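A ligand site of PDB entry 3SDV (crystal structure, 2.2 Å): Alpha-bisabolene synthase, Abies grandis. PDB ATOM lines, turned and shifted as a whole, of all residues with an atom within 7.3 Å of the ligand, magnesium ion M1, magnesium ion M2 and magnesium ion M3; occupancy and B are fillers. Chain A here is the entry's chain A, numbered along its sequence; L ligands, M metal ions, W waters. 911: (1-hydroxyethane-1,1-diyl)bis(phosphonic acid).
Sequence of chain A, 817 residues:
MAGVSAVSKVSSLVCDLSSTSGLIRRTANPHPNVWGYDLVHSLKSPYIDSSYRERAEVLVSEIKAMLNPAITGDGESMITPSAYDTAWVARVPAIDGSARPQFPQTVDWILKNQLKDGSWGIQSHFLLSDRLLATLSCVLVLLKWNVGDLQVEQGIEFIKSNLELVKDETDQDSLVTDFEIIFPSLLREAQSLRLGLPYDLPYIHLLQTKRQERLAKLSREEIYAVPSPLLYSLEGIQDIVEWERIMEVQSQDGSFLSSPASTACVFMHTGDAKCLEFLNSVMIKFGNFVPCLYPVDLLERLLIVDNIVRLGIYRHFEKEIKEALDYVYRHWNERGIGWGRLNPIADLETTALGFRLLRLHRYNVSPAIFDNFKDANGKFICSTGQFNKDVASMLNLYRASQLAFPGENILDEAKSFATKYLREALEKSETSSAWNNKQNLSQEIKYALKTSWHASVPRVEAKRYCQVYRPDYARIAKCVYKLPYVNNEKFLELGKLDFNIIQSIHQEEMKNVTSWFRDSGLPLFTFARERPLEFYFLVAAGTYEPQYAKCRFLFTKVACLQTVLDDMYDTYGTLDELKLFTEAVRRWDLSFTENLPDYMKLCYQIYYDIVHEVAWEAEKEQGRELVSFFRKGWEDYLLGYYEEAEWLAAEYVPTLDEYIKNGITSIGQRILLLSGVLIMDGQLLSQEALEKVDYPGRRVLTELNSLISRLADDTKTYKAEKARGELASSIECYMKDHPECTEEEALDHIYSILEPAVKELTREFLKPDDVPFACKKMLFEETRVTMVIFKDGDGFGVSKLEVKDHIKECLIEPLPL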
ATOM      1  N   ARG A 531     -25.080  27.757  -6.098  1.00  0.00           N
ATOM      2  CA  ARG A 531     -23.621  27.635  -6.030  1.00  0.00           C
ATOM      3  C   ARG A 531     -22.903  27.857  -7.360  1.00  0.00           C
ATOM      4  O   ARG A 531     -21.931  27.168  -7.672  1.00  0.00           O
ATOM      5  CB  ARG A 531     -23.226  26.257  -5.470  1.00  0.00           C
ATOM      6  CG  ARG A 531     -23.818  25.937  -4.110  1.00  0.00           C
ATOM      7  CD  ARG A 531     -23.199  24.679  -3.528  1.00  0.00           C
ATOM      8  NE  ARG A 531     -23.692  23.453  -4.150  1.00  0.00           N
ATOM      9  CZ  ARG A 531     -22.989  22.333  -4.229  1.00  0.00           C
ATOM     10  NH1 ARG A 531     -21.762  22.278  -3.734  1.00  0.00           N
ATOM     11  NH2 ARG A 531     -23.513  21.251  -4.806  1.00  0.00           N
ATOM     12  N   THR A 563     -27.466  20.268  -9.342  1.00  0.00           N
ATOM     13  CA  THR A 563     -27.622  20.398  -7.905  1.00  0.00           C
ATOM     14  C   THR A 563     -29.095  20.521  -7.529  1.00  0.00           C
ATOM     15  O   THR A 563     -29.518  20.037  -6.481  1.00  0.00           O
ATOM     16  CB  THR A 563     -26.803  21.580  -7.330  1.00  0.00           C
ATOM     17  OG1 THR A 563     -26.806  21.519  -5.902  1.00  0.00           O
ATOM     18  CG2 THR A 563     -27.362  22.925  -7.778  1.00  0.00           C
ATOM     19  N   LEU A 565     -31.608  19.192  -9.536  1.00  0.00           N
ATOM     20  CA  LEU A 565     -32.119  17.858  -9.830  1.00  0.00           C
ATOM     21  C   LEU A 565     -31.797  16.912  -8.679  1.00  0.00           C
ATOM     22  O   LEU A 565     -32.630  16.085  -8.295  1.00  0.00           O
ATOM     23  CB  LEU A 565     -31.521  17.327 -11.148  1.00  0.00           C
ATOM     24  CG  LEU A 565     -31.947  18.038 -12.437  1.00  0.00           C
ATOM     25  CD1 LEU A 565     -31.259  17.429 -13.640  1.00  0.00           C
ATOM     26  CD2 LEU A 565     -33.462  17.967 -12.588  1.00  0.00           C
ATOM     27  N   ASP A 566     -30.606  17.051  -8.119  1.00  0.00           N
ATOM     28  CA  ASP A 566     -30.160  16.187  -7.036  1.00  0.00           C
ATOM     29  C   ASP A 566     -31.036  16.356  -5.793  1.00  0.00           C
ATOM     30  O   ASP A 566     -31.512  15.376  -5.229  1.00  0.00           O
ATOM     31  CB  ASP A 566     -28.680  16.423  -6.694  1.00  0.00           C
ATOM     32  CG  ASP A 566     -28.179  15.480  -5.593  1.00  0.00           C
ATOM     33  OD1 ASP A 566     -28.312  14.254  -5.764  1.00  0.00           O
ATOM     34  OD2 ASP A 566     -27.681  15.969  -4.548  1.00  0.00           O
ATOM     35  N   ASP A 567     -31.238  17.604  -5.364  1.00  0.00           N
ATOM     36  CA  ASP A 567     -32.028  17.892  -4.174  1.00  0.00           C
ATOM     37  C   ASP A 567     -33.486  17.525  -4.395  1.00  0.00           C
ATOM     38  O   ASP A 567     -34.195  17.162  -3.457  1.00  0.00           O
ATOM     39  CB  ASP A 567     -31.908  19.360  -3.757  1.00  0.00           C
ATOM     40  CG  ASP A 567     -30.489  19.748  -3.365  1.00  0.00           C
ATOM     41  OD1 ASP A 567     -29.653  18.842  -3.169  1.00  0.00           O
ATOM     42  OD2 ASP A 567     -30.204  20.951  -3.245  1.00  0.00           O
ATOM     43  N   MET A 568     -33.929  17.616  -5.642  1.00  0.00           N
ATOM     44  CA  MET A 568     -35.297  17.218  -5.972  1.00  0.00           C
ATOM     45  C   MET A 568     -35.494  15.714  -5.792  1.00  0.00           C
ATOM     46  O   MET A 568     -36.493  15.259  -5.224  1.00  0.00           O
ATOM     47  CB  MET A 568     -35.641  17.633  -7.413  1.00  0.00           C
ATOM     48  CG  MET A 568     -37.113  17.506  -7.775  1.00  0.00           C
ATOM     49  SD  MET A 568     -37.445  18.002  -9.478  1.00  0.00           S
ATOM     50  CE  MET A 568     -36.629  16.679 -10.362  1.00  0.00           C
ATOM     51  N   TYR A 569     -34.528  14.928  -6.262  1.00  0.00           N
ATOM     52  CA  TYR A 569     -34.641  13.477  -6.216  1.00  0.00           C
ATOM     53  C   TYR A 569     -34.342  12.869  -4.849  1.00  0.00           C
ATOM     54  O   TYR A 569     -34.981  11.900  -4.468  1.00  0.00           O
ATOM     55  CB  TYR A 569     -33.752  12.823  -7.265  1.00  0.00           C
ATOM     56  CG  TYR A 569     -34.441  12.601  -8.591  1.00  0.00           C
ATOM     57  CD1 TYR A 569     -35.110  11.413  -8.847  1.00  0.00           C
ATOM     58  CD2 TYR A 569     -34.411  13.576  -9.574  1.00  0.00           C
ATOM     59  CE1 TYR A 569     -35.739  11.199 -10.064  1.00  0.00           C
ATOM     60  CE2 TYR A 569     -35.034  13.374 -10.789  1.00  0.00           C
ATOM     61  CZ  TYR A 569     -35.704  12.185 -11.031  1.00  0.00           C
ATOM     62  OH  TYR A 569     -36.326  11.982 -12.245  1.00  0.00           O
ATOM     63  N   ASP A 570     -33.351  13.399  -4.143  1.00  0.00           N
ATOM     64  CA  ASP A 570     -32.997  12.762  -2.874  1.00  0.00           C
ATOM     65  C   ASP A 570     -33.611  13.417  -1.627  1.00  0.00           C
ATOM     66  O   ASP A 570     -33.575  12.843  -0.545  1.00  0.00           O
ATOM     67  CB  ASP A 570     -31.485  12.482  -2.729  1.00  0.00           C
ATOM     68  CG  ASP A 570     -30.610  13.717  -2.851  1.00  0.00           C
ATOM     69  OD1 ASP A 570     -30.989  14.795  -2.345  1.00  0.00           O
ATOM     70  OD2 ASP A 570     -29.503  13.598  -3.435  1.00  0.00           O
ATOM     71  N   THR A 571     -34.218  14.583  -1.803  1.00  0.00           N
ATOM     72  CA  THR A 571     -34.785  15.328  -0.675  1.00  0.00           C
ATOM     73  C   THR A 571     -36.226  15.776  -0.911  1.00  0.00           C
ATOM     74  O   THR A 571     -37.161  15.257  -0.302  1.00  0.00           O
ATOM     75  CB  THR A 571     -33.913  16.547  -0.312  1.00  0.00           C
ATOM     76  OG1 THR A 571     -32.575  16.122  -0.055  1.00  0.00           O
ATOM     77  CG2 THR A 571     -34.462  17.250   0.921  1.00  0.00           C
ATOM     78  N   TYR A 641     -30.949   8.254 -10.477  1.00  0.00           N
ATOM     79  CA  TYR A 641     -31.564   8.994  -9.391  1.00  0.00           C
ATOM     80  C   TYR A 641     -32.864   8.330  -8.923  1.00  0.00           C
ATOM     81  O   TYR A 641     -33.089   8.159  -7.730  1.00  0.00           O
ATOM     82  CB  TYR A 641     -31.904  10.410  -9.846  1.00  0.00           C
ATOM     83  CG  TYR A 641     -30.817  11.435  -9.621  1.00  0.00           C
ATOM     84  CD1 TYR A 641     -29.714  11.155  -8.812  1.00  0.00           C
ATOM     85  CD2 TYR A 641     -30.896  12.678 -10.206  1.00  0.00           C
ATOM     86  CE1 TYR A 641     -28.722  12.101  -8.616  1.00  0.00           C
ATOM     87  CE2 TYR A 641     -29.910  13.631 -10.024  1.00  0.00           C
ATOM     88  CZ  TYR A 641     -28.834  13.344  -9.227  1.00  0.00           C
ATOM     89  OH  TYR A 641     -27.874  14.313  -9.046  1.00  0.00           O
ATOM     90  N   GLU A 644     -32.415   5.155  -6.980  1.00  0.00           N
ATOM     91  CA  GLU A 644     -32.020   5.587  -5.645  1.00  0.00           C
ATOM     92  C   GLU A 644     -33.230   6.123  -4.879  1.00  0.00           C
ATOM     93  O   GLU A 644     -33.372   5.898  -3.669  1.00  0.00           O
ATOM     94  CB  GLU A 644     -30.929   6.660  -5.743  1.00  0.00           C
ATOM     95  CG  GLU A 644     -30.258   7.023  -4.436  1.00  0.00           C
ATOM     96  CD  GLU A 644     -29.089   7.988  -4.641  1.00  0.00           C
ATOM     97  OE1 GLU A 644     -28.105   7.913  -3.868  1.00  0.00           O
ATOM     98  OE2 GLU A 644     -29.161   8.819  -5.562  1.00  0.00           O
ATOM     99  N   TYR A 659     -24.793  -0.617  -4.799  1.00  0.00           N
ATOM    100  CA  TYR A 659     -24.563   0.778  -4.472  1.00  0.00           C
ATOM    101  C   TYR A 659     -23.583   1.411  -5.434  1.00  0.00           C
ATOM    102  O   TYR A 659     -23.799   2.509  -5.933  1.00  0.00           O
ATOM    103  CB  TYR A 659     -24.031   0.901  -3.056  1.00  0.00           C
ATOM    104  CG  TYR A 659     -23.744   2.316  -2.627  1.00  0.00           C
ATOM    105  CD1 TYR A 659     -24.746   3.088  -2.027  1.00  0.00           C
ATOM    106  CD2 TYR A 659     -22.504   2.880  -2.806  1.00  0.00           C
ATOM    107  CE1 TYR A 659     -24.501   4.376  -1.627  1.00  0.00           C
ATOM    108  CE2 TYR A 659     -22.239   4.181  -2.409  1.00  0.00           C
ATOM    109  CZ  TYR A 659     -23.249   4.919  -1.822  1.00  0.00           C
ATOM    110  OH  TYR A 659     -23.010   6.217  -1.414  1.00  0.00           O
ATOM    111  N   SER A 666     -25.416   7.566 -11.153  1.00  0.00           N
ATOM    112  CA  SER A 666     -26.290   8.603 -10.624  1.00  0.00           C
ATOM    113  C   SER A 666     -25.555   9.767  -9.961  1.00  0.00           C
ATOM    114  O   SER A 666     -26.183  10.772  -9.630  1.00  0.00           O
ATOM    115  CB  SER A 666     -27.281   8.011  -9.621  1.00  0.00           C
ATOM    116  OG  SER A 666     -26.638   7.769  -8.387  1.00  0.00           O
ATOM    117  N   ILE A 667     -24.250   9.650  -9.759  1.00  0.00           N
ATOM    118  CA  ILE A 667     -23.546  10.779  -9.162  1.00  0.00           C
ATOM    119  C   ILE A 667     -23.443  11.911 -10.180  1.00  0.00           C
ATOM    120  O   ILE A 667     -23.230  13.067  -9.823  1.00  0.00           O
ATOM    121  CB  ILE A 667     -22.185  10.411  -8.558  1.00  0.00           C
ATOM    122  CG1 ILE A 667     -21.648  11.605  -7.749  1.00  0.00           C
ATOM    123  CG2 ILE A 667     -21.190   9.986  -9.635  1.00  0.00           C
ATOM    124  CD1 ILE A 667     -20.439  11.306  -6.915  1.00  0.00           C
ATOM    125  N   SER A 709     -15.277  10.064  -7.359  1.00  0.00           N
ATOM    126  CA  SER A 709     -16.126  11.103  -6.791  1.00  0.00           C
ATOM    127  C   SER A 709     -17.092  10.516  -5.763  1.00  0.00           C
ATOM    128  O   SER A 709     -17.190  11.012  -4.643  1.00  0.00           O
ATOM    129  CB  SER A 709     -16.928  11.823  -7.885  1.00  0.00           C
ATOM    130  OG  SER A 709     -16.071  12.427  -8.837  1.00  0.00           O
ATOM    131  N   ARG A 710     -17.807   9.477  -6.155  1.00  0.00           N
ATOM    132  CA  ARG A 710     -18.761   8.826  -5.264  1.00  0.00           C
ATOM    133  C   ARG A 710     -18.100   8.406  -3.951  1.00  0.00           C
ATOM    134  O   ARG A 710     -18.585   8.725  -2.872  1.00  0.00           O
ATOM    135  CB  ARG A 710     -19.392   7.618  -5.971  1.00  0.00           C
ATOM    136  CG  ARG A 710     -20.325   6.769  -5.113  1.00  0.00           C
ATOM    137  CD  ARG A 710     -21.636   7.478  -4.845  1.00  0.00           C
ATOM    138  NE  ARG A 710     -21.515   8.445  -3.756  1.00  0.00           N
ATOM    139  CZ  ARG A 710     -22.370   9.456  -3.559  1.00  0.00           C
ATOM    140  NH1 ARG A 710     -23.386   9.647  -4.392  1.00  0.00           N
ATOM    141  NH2 ARG A 710     -22.169  10.282  -2.545  1.00  0.00           N
ATOM    142  N   ASP A 713     -16.427  11.183  -1.871  1.00  0.00           N
ATOM    143  CA  ASP A 713     -17.554  11.832  -1.202  1.00  0.00           C
ATOM    144  C   ASP A 713     -17.951  11.055   0.053  1.00  0.00           C
ATOM    145  O   ASP A 713     -18.041  11.621   1.140  1.00  0.00           O
ATOM    146  CB  ASP A 713     -18.755  11.964  -2.144  1.00  0.00           C
ATOM    147  CG  ASP A 713     -19.894  12.778  -1.547  1.00  0.00           C
ATOM    148  OD1 ASP A 713     -20.275  12.545  -0.373  1.00  0.00           O
ATOM    149  OD2 ASP A 713     -20.419  13.667  -2.241  1.00  0.00           O
ATOM    150  N   ASP A 714     -18.209   9.759  -0.106  1.00  0.00           N
ATOM    151  CA  ASP A 714     -18.595   8.940   1.037  1.00  0.00           C
ATOM    152  C   ASP A 714     -17.597   9.005   2.183  1.00  0.00           C
ATOM    153  O   ASP A 714     -17.972   9.201   3.337  1.00  0.00           O
ATOM    154  CB  ASP A 714     -18.826   7.481   0.615  1.00  0.00           C
ATOM    155  CG  ASP A 714     -20.121   7.295  -0.137  1.00  0.00           C
ATOM    156  OD1 ASP A 714     -20.930   8.253  -0.179  1.00  0.00           O
ATOM    157  OD2 ASP A 714     -20.347   6.185  -0.676  1.00  0.00           O
ATOM    158  N   THR A 717     -17.770  12.427   3.935  1.00  0.00           N
ATOM    159  CA  THR A 717     -19.010  12.663   4.663  1.00  0.00           C
ATOM    160  C   THR A 717     -19.529  11.366   5.300  1.00  0.00           C
ATOM    161  O   THR A 717     -18.913  10.831   6.211  1.00  0.00           O
ATOM    162  CB  THR A 717     -20.082  13.296   3.762  1.00  0.00           C
ATOM    163  OG1 THR A 717     -20.285  12.478   2.598  1.00  0.00           O
ATOM    164  CG2 THR A 717     -19.637  14.674   3.307  1.00  0.00           C
ATOM    165  N   TYR A 718     -20.651  10.863   4.805  1.00  0.00           N
ATOM    166  CA  TYR A 718     -21.208   9.593   5.305  1.00  0.00           C
ATOM    167  C   TYR A 718     -21.623   9.646   6.780  1.00  0.00           C
ATOM    168  O   TYR A 718     -22.684   9.136   7.146  1.00  0.00           O
ATOM    169  CB  TYR A 718     -20.252   8.418   5.039  1.00  0.00           C
ATOM    170  CG  TYR A 718     -19.587   7.827   6.272  1.00  0.00           C
ATOM    171  CD1 TYR A 718     -18.254   8.126   6.577  1.00  0.00           C
ATOM    172  CD2 TYR A 718     -20.270   6.965   7.115  1.00  0.00           C
ATOM    173  CE1 TYR A 718     -17.649   7.585   7.701  1.00  0.00           C
ATOM    174  CE2 TYR A 718     -19.664   6.424   8.239  1.00  0.00           C
ATOM    175  CZ  TYR A 718     -18.356   6.740   8.530  1.00  0.00           C
ATOM    176  OH  TYR A 718     -17.748   6.202   9.640  1.00  0.00           O
ATOM    177  N   LEU A 727     -29.888   8.383   3.792  1.00  0.00           N
ATOM    178  CA  LEU A 727     -30.324   7.021   3.539  1.00  0.00           C
ATOM    179  C   LEU A 727     -29.271   5.985   3.972  1.00  0.00           C
ATOM    180  O   LEU A 727     -29.398   5.393   5.047  1.00  0.00           O
ATOM    181  CB  LEU A 727     -30.715   6.818   2.064  1.00  0.00           C
ATOM    182  CG  LEU A 727     -29.746   7.134   0.920  1.00  0.00           C
ATOM    183  CD1 LEU A 727     -30.298   6.581  -0.384  1.00  0.00           C
ATOM    184  CD2 LEU A 727     -29.473   8.632   0.792  1.00  0.00           C
ATOM    185  N   PHE A 790     -12.940  16.942  -1.482  1.00  0.00           N
ATOM    186  CA  PHE A 790     -13.229  15.844  -0.568  1.00  0.00           C
ATOM    187  C   PHE A 790     -12.008  15.232   0.123  1.00  0.00           C
ATOM    188  O   PHE A 790     -12.072  14.096   0.606  1.00  0.00           O
ATOM    189  CB  PHE A 790     -14.018  14.742  -1.286  1.00  0.00           C
ATOM    190  CG  PHE A 790     -15.341  15.195  -1.809  1.00  0.00           C
ATOM    191  CD1 PHE A 790     -16.352  15.583  -0.947  1.00  0.00           C
ATOM    192  CD2 PHE A 790     -15.573  15.242  -3.174  1.00  0.00           C
ATOM    193  CE1 PHE A 790     -17.571  16.017  -1.433  1.00  0.00           C
ATOM    194  CE2 PHE A 790     -16.799  15.664  -3.662  1.00  0.00           C
ATOM    195  CZ  PHE A 790     -17.798  16.051  -2.791  1.00  0.00           C
HETATM  196  P1  911 L   1     -24.861  15.625  -1.880  1.00  0.00           P
HETATM  197  O2  911 L   1     -23.803  16.755  -2.075  1.00  0.00           O
HETATM  198  O3  911 L   1     -24.787  15.154  -0.398  1.00  0.00           O
HETATM  199  O5  911 L   1     -26.244  16.087  -2.230  1.00  0.00           O
HETATM  200  C7  911 L   1     -24.373  14.181  -2.884  1.00  0.00           C
HETATM  201  P8  911 L   1     -25.683  12.922  -2.794  1.00  0.00           P
HETATM  202  O9  911 L   1     -27.047  13.470  -3.165  1.00  0.00           O
HETATM  203  O10 911 L   1     -25.261  11.757  -3.738  1.00  0.00           O
HETATM  204  O12 911 L   1     -25.640  12.399  -1.330  1.00  0.00           O
HETATM  205  O14 911 L   1     -23.239  13.632  -2.324  1.00  0.00           O
HETATM  206  C16 911 L   1     -24.110  14.594  -4.298  1.00  0.00           C
HETATM  207 MG    MG M   1     -28.500  15.255  -2.493  1.00  0.00          MG
HETATM  208 MG    MG M   2     -24.097  13.200   0.060  1.00  0.00          MG
HETATM  209 MG    MG M   3     -28.240  12.439  -4.546  1.00  0.00          MG
HETATM  210  O   HOH W   1     -29.834  12.003  -5.849  1.00  0.00           O
HETATM  211  O   HOH W   2     -22.435  13.491   1.258  1.00  0.00           O
HETATM  212  O   HOH W   3     -28.711  17.006  -1.393  1.00  0.00           O
HETATM  213  O   HOH W   4     -28.487  10.772  -3.361  1.00  0.00           O
HETATM  214  O   HOH W   5     -27.951  14.490  -0.616  1.00  0.00           O
HETATM  215  O   HOH W   6     -24.017  11.161  -0.247  1.00  0.00           O
HETATM  216  O   HOH W   7     -26.927  11.412  -5.792  1.00  0.00           O
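O10 of the ligand lies within salt-bridge range of NH1 of Arg 710, 2.9 Å away.
The side-chain carboxylate (OD2) of Asp 713 lies close to an oxygen (O14) of the ligand, at 2.8 Å.
The side-chain carboxylate (OD1) of Asp 566 lies close to the side-chain hydroxyl (OH) of Tyr 641, at 3.3 Å.
OG1 of Thr 571 sits close to OD1 of Asp 570 (3.1 Å).
OG1 of Thr 717 lies within hydrogen-bond range of O of Asp 713, 2.8 Å away.
The guanidinium group of Arg 710 lies within salt-bridge range of the side-chain carboxylate of Asp 714.
The side-chain carboxylate of Asp 713 lies within salt-bridge range of the guanidinium group of Arg 710 (3.7 Å).
Of the 22 residues printed, 4 come within 4 Å of the ligand.
The nearest printed residue that does not touch the ligand is Asp 567 (4.5 Å).
OD1 of Asp 567 touches magnesium ion M1, at 3.8 Å.
Asp 713 touches magnesium ion M2.
Of the 22 residues printed, 1 comes within 4 Å of magnesium ion M2.
Merely in contact with magnesium ion M3: Glu 644.
Along chain A the residues within 4 Å of magnesium ion M3 span positions 566 to 644.
The nearest printed residue that does not touch magnesium ion M3 is Tyr 641 (4.1 Å).
Magnesium ion M1 is bound by water W3 (2.1 Å), water W5 (2.1 Å), the side-chain carboxylate (OD2) of Asp 570 (2.2 Å), the side-chain carboxylate (OD2) of Asp 566 (2.3 Å), an oxygen (O9) of the ligand (2.4 Å), an oxygen (O5) of the ligand (2.4 Å) and the side-chain carboxylate (OD1) of Asp 570 (2.5 Å).
Magnesium ion M1 has seven donor atoms within binding distance.
Magnesium ion M2 is bound by water W6 (2.1 Å), water W2 (2.1 Å), O3 of the ligand (2.1 Å), O12 of the ligand (2.2 Å) and O14 of the ligand (2.6 Å).
Magnesium ion M2 has five donor atoms within binding distance.
OD2 of Asp 570 is bound to magnesium ion M3 (2.0 Å).
Water W4 binds magnesium ion M3, at 2.1 Å.
Water W7 binds magnesium ion M3.
Magnesium ion M3 is bound by O9 of the ligand (2.1 Å).
Water W1 is bound to magnesium ion M3.
OD1 of Asp 566 is bound to magnesium ion M3.
Magnesium ion M3 has six donor atoms within binding distance.
Water W2 bridges OG1 of Thr 717 (2.7 Å) and OD1 of Asp 713 (2.9 Å).
Water W7 lies within hydrogen-bond range of an oxygen (O10) of the ligand (2.7 Å) and the side-chain carboxylate of Glu 644 (3.4 Å).
Water W4 bridges the side-chain carboxylate of Glu 644 (2.9 Å) and an oxygen (O10) of the ligand (3.4 Å).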
